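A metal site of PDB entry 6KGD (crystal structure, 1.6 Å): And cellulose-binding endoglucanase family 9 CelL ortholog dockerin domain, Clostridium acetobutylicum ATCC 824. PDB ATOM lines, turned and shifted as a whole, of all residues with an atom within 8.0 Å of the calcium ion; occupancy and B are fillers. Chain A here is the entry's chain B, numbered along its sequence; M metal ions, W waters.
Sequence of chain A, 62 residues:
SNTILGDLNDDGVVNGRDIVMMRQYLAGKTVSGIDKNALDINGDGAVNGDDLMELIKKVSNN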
ATOM      1  N   GLY A   6       3.926  23.496 -10.146  1.00  0.00           N
ATOM      2  CA  GLY A   6       3.450  23.978 -11.440  1.00  0.00           C
ATOM      3  C   GLY A   6       3.166  22.900 -12.481  1.00  0.00           C
ATOM      4  O   GLY A   6       3.208  23.152 -13.687  1.00  0.00           O
ATOM      5  N   ASP A   7       2.857  21.688 -12.016  1.00  0.00           N
ATOM      6  CA  ASP A   7       2.609  20.565 -12.912  1.00  0.00           C
ATOM      7  C   ASP A   7       1.108  20.493 -13.164  1.00  0.00           C
ATOM      8  O   ASP A   7       0.363  19.707 -12.561  1.00  0.00           O
ATOM      9  CB  ASP A   7       3.155  19.276 -12.324  1.00  0.00           C
ATOM     10  CG  ASP A   7       2.857  18.068 -13.172  1.00  0.00           C
ATOM     11  OD1 ASP A   7       2.610  18.226 -14.388  1.00  0.00           O
ATOM     12  OD2 ASP A   7       2.874  16.944 -12.631  1.00  0.00           O
ATOM     13  N   LEU A   8       0.649  21.348 -14.072  1.00  0.00           N
ATOM     14  CA  LEU A   8      -0.768  21.609 -14.192  1.00  0.00           C
ATOM     15  C   LEU A   8      -1.489  20.440 -14.848  1.00  0.00           C
ATOM     16  O   LEU A   8      -2.688  20.228 -14.609  1.00  0.00           O
ATOM     17  CB  LEU A   8      -1.007  22.879 -14.982  1.00  0.00           C
ATOM     18  CG  LEU A   8      -0.358  24.195 -14.493  1.00  0.00           C
ATOM     19  CD1 LEU A   8      -1.032  25.353 -15.224  1.00  0.00           C
ATOM     20  CD2 LEU A   8      -0.414  24.373 -13.002  1.00  0.00           C
ATOM     21  N   ASN A   9      -0.813  19.678 -15.693  1.00  0.00           N
ATOM     22  CA  ASN A   9      -1.443  18.520 -16.323  1.00  0.00           C
ATOM     23  C   ASN A   9      -1.090  17.230 -15.609  1.00  0.00           C
ATOM     24  O   ASN A   9      -1.421  16.149 -16.118  1.00  0.00           O
ATOM     25  CB  ASN A   9      -1.048  18.441 -17.786  1.00  0.00           C
ATOM     26  CG  ASN A   9       0.449  18.354 -17.975  1.00  0.00           C
ATOM     27  OD1 ASN A   9       1.198  18.205 -17.021  1.00  0.00           O
ATOM     28  ND2 ASN A   9       0.880  18.472 -19.214  1.00  0.00           N
ATOM     29  N   ASP A  10      -0.398  17.314 -14.480  1.00  0.00           N
ATOM     30  CA  ASP A  10      -0.120  16.169 -13.609  1.00  0.00           C
ATOM     31  C   ASP A  10       0.504  15.008 -14.379  1.00  0.00           C
ATOM     32  O   ASP A  10       0.089  13.857 -14.254  1.00  0.00           O
ATOM     33  CB  ASP A  10      -1.385  15.711 -12.886  1.00  0.00           C
ATOM     34  CG  ASP A  10      -1.108  14.645 -11.856  1.00  0.00           C
ATOM     35  OD1 ASP A  10      -0.197  14.845 -11.021  1.00  0.00           O
ATOM     36  OD2 ASP A  10      -1.792  13.598 -11.883  1.00  0.00           O
ATOM     37  N   ASP A  11       1.531  15.314 -15.181  1.00  0.00           N
ATOM     38  CA  ASP A  11       2.304  14.286 -15.854  1.00  0.00           C
ATOM     39  C   ASP A  11       3.673  14.052 -15.210  1.00  0.00           C
ATOM     40  O   ASP A  11       4.441  13.222 -15.689  1.00  0.00           O
ATOM     41  CB  ASP A  11       2.436  14.609 -17.359  1.00  0.00           C
ATOM     42  CG  ASP A  11       3.273  15.851 -17.661  1.00  0.00           C
ATOM     43  OD1 ASP A  11       3.809  16.512 -16.733  1.00  0.00           O
ATOM     44  OD2 ASP A  11       3.407  16.170 -18.870  1.00  0.00           O
ATOM     45  N   GLY A  12       3.976  14.753 -14.114  1.00  0.00           N
ATOM     46  CA  GLY A  12       5.198  14.509 -13.370  1.00  0.00           C
ATOM     47  C   GLY A  12       6.355  15.423 -13.713  1.00  0.00           C
ATOM     48  O   GLY A  12       7.387  15.359 -13.040  1.00  0.00           O
ATOM     49  N   VAL A  13       6.226  16.250 -14.740  1.00  0.00           N
ATOM     50  CA  VAL A  13       7.278  17.181 -15.112  1.00  0.00           C
ATOM     51  C   VAL A  13       6.660  18.558 -15.253  1.00  0.00           C
ATOM     52  O   VAL A  13       5.455  18.687 -15.522  1.00  0.00           O
ATOM     53  CB  VAL A  13       8.016  16.783 -16.408  1.00  0.00           C
ATOM     54  CG1 VAL A  13       8.764  15.484 -16.218  1.00  0.00           C
ATOM     55  CG2 VAL A  13       7.037  16.688 -17.561  1.00  0.00           C
ATOM     56  N   VAL A  14       7.490  19.568 -15.065  1.00  0.00           N
ATOM     57  CA  VAL A  14       7.102  20.950 -15.309  1.00  0.00           C
ATOM     58  C   VAL A  14       7.825  21.404 -16.559  1.00  0.00           C
ATOM     59  O   VAL A  14       9.060  21.505 -16.580  1.00  0.00           O
ATOM     60  CB  VAL A  14       7.438  21.859 -14.105  1.00  0.00           C
ATOM     61  CG1 VAL A  14       6.987  23.266 -14.406  1.00  0.00           C
ATOM     62  CG2 VAL A  14       6.759  21.338 -12.853  1.00  0.00           C
ATOM     63  N   ASN A  15       7.060  21.705 -17.603  1.00  0.00           N
ATOM     64  CA  ASN A  15       7.639  22.037 -18.884  1.00  0.00           C
ATOM     65  C   ASN A  15       6.659  22.907 -19.656  1.00  0.00           C
ATOM     66  O   ASN A  15       5.693  23.442 -19.110  1.00  0.00           O
ATOM     67  CB  ASN A  15       8.021  20.769 -19.667  1.00  0.00           C
ATOM     68  CG  ASN A  15       6.837  19.907 -20.068  1.00  0.00           C
ATOM     69  OD1 ASN A  15       5.676  20.342 -20.090  1.00  0.00           O
ATOM     70  ND2 ASN A  15       7.128  18.665 -20.408  1.00  0.00           N
ATOM     71  N   GLY A  16       6.941  23.096 -20.934  1.00  0.00           N
ATOM     72  CA  GLY A  16       6.162  24.034 -21.722  1.00  0.00           C
ATOM     73  C   GLY A  16       4.692  23.685 -21.852  1.00  0.00           C
ATOM     74  O   GLY A  16       3.862  24.575 -22.058  1.00  0.00           O
ATOM     75  N   ARG A  17       4.334  22.404 -21.730  1.00  0.00           N
ATOM     76  CA  ARG A  17       2.910  22.059 -21.741  1.00  0.00           C
ATOM     77  C   ARG A  17       2.181  22.759 -20.596  1.00  0.00           C
ATOM     78  O   ARG A  17       1.052  23.218 -20.756  1.00  0.00           O
ATOM     79  CB  ARG A  17       2.710  20.563 -21.643  1.00  0.00           C
ATOM     80  CG  ARG A  17       3.274  19.751 -22.779  1.00  0.00           C
ATOM     81  CD  ARG A  17       2.787  18.324 -22.634  1.00  0.00           C
ATOM     82  NE  ARG A  17       3.339  17.330 -23.534  1.00  0.00           N
ATOM     83  CZ  ARG A  17       2.963  17.139 -24.784  1.00  0.00           C
ATOM     84  NH1 ARG A  17       2.074  17.945 -25.349  1.00  0.00           N
ATOM     85  NH2 ARG A  17       3.504  16.147 -25.491  1.00  0.00           N
ATOM     86  N   ASP A  18       2.815  22.820 -19.428  1.00  0.00           N
ATOM     87  CA  ASP A  18       2.215  23.472 -18.270  1.00  0.00           C
ATOM     88  C   ASP A  18       2.078  24.964 -18.490  1.00  0.00           C
ATOM     89  O   ASP A  18       1.103  25.581 -18.054  1.00  0.00           O
ATOM     90  CB  ASP A  18       3.058  23.174 -17.036  1.00  0.00           C
ATOM     91  CG  ASP A  18       3.169  21.696 -16.771  1.00  0.00           C
ATOM     92  OD1 ASP A  18       2.131  21.054 -16.497  1.00  0.00           O
ATOM     93  OD2 ASP A  18       4.279  21.167 -16.867  1.00  0.00           O
ATOM     94  N   ILE A  19       3.072  25.584 -19.156  1.00  0.00           N
ATOM     95  CA  ILE A  19       2.961  27.005 -19.479  1.00  0.00           C
ATOM     96  C   ILE A  19       1.770  27.278 -20.381  1.00  0.00           C
ATOM     97  O   ILE A  19       1.002  28.225 -20.170  1.00  0.00           O
ATOM     98  CB  ILE A  19       4.275  27.509 -20.098  1.00  0.00           C
ATOM     99  CG1 ILE A  19       5.398  27.422 -19.080  1.00  0.00           C
ATOM    100  CG2 ILE A  19       4.098  28.942 -20.608  1.00  0.00           C
ATOM    101  CD1 ILE A  19       6.774  27.806 -19.635  1.00  0.00           C
ATOM    102  N   MET A  21      -0.960  25.606 -20.673  1.00  0.00           N
ATOM    103  CA  MET A  21      -2.212  25.430 -19.940  1.00  0.00           C
ATOM    104  C   MET A  21      -2.470  26.603 -19.007  1.00  0.00           C
ATOM    105  O   MET A  21      -3.615  27.066 -18.896  1.00  0.00           O
ATOM    106  CB  MET A  21      -2.210  24.118 -19.178  1.00  0.00           C
ATOM    107  CG  MET A  21      -2.268  22.941 -20.106  1.00  0.00           C
ATOM    108  SD  MET A  21      -2.272  21.424 -19.149  1.00  0.00           S
ATOM    109  CE  MET A  21      -3.828  21.560 -18.293  1.00  0.00           C
ATOM    110  N   LEU A  55       6.033  29.980 -12.851  1.00  0.00           N
ATOM    111  CA  LEU A  55       6.129  28.783 -13.674  1.00  0.00           C
ATOM    112  C   LEU A  55       7.219  28.944 -14.716  1.00  0.00           C
ATOM    113  O   LEU A  55       8.043  28.039 -14.915  1.00  0.00           O
ATOM    114  CB  LEU A  55       4.771  28.523 -14.314  1.00  0.00           C
ATOM    115  CG  LEU A  55       4.664  27.373 -15.303  1.00  0.00           C
ATOM    116  CD1 LEU A  55       5.184  26.091 -14.699  1.00  0.00           C
ATOM    117  CD2 LEU A  55       3.229  27.241 -15.758  1.00  0.00           C
HETATM  118 CA    CA M   1       3.416  18.899 -16.496  1.00  0.00          CA
HETATM  119  O   HOH W   1       3.851  18.757 -18.825  1.00  0.00           O
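The side-chain carboxylate (OD1) of Asp 7 lies close to the backbone NH (N) of Asp 10 (3.1 Å).
The backbone NH (N) of Gly 12 is in hydrogen-bond range of the side-chain carboxylate (OD2) of Asp 7 (2.9 Å).
OD1 of Asp 18 lies close to N of Leu 8 (2.9 Å).
The side-chain carboxylate (OD2) of Asp 18 sits close to the backbone NH (N) of Asn 15.
Along chain A the residues within 4 Å of the calcium ion span positions 7 to 18.
The backbone carbonyl oxygen (O) of Val 13 is bound to the calcium ion (2.3 Å).
The calcium ion is bound by OD1 of Asp 7.
The calcium ion is bound by water W1 (2.4 Å).
The calcium ion is bound by the side-chain amide oxygen (OD1) of Asn 9 (2.4 Å).
OD1 of Asp 11 binds the calcium ion (2.4 Å).
OD2 of Asp 18 is bound to the calcium ion (2.5 Å).
OD1 of Asp 18 binds the calcium ion (2.5 Å).
The calcium ion has seven donor atoms within binding distance.
Water W1 lies within hydrogen-bond range of OD2 of Asp 11 (2.6 Å), OD1 of Asn 15 (2.7 Å) and ND2 of Asn 9 (3.0 Å).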
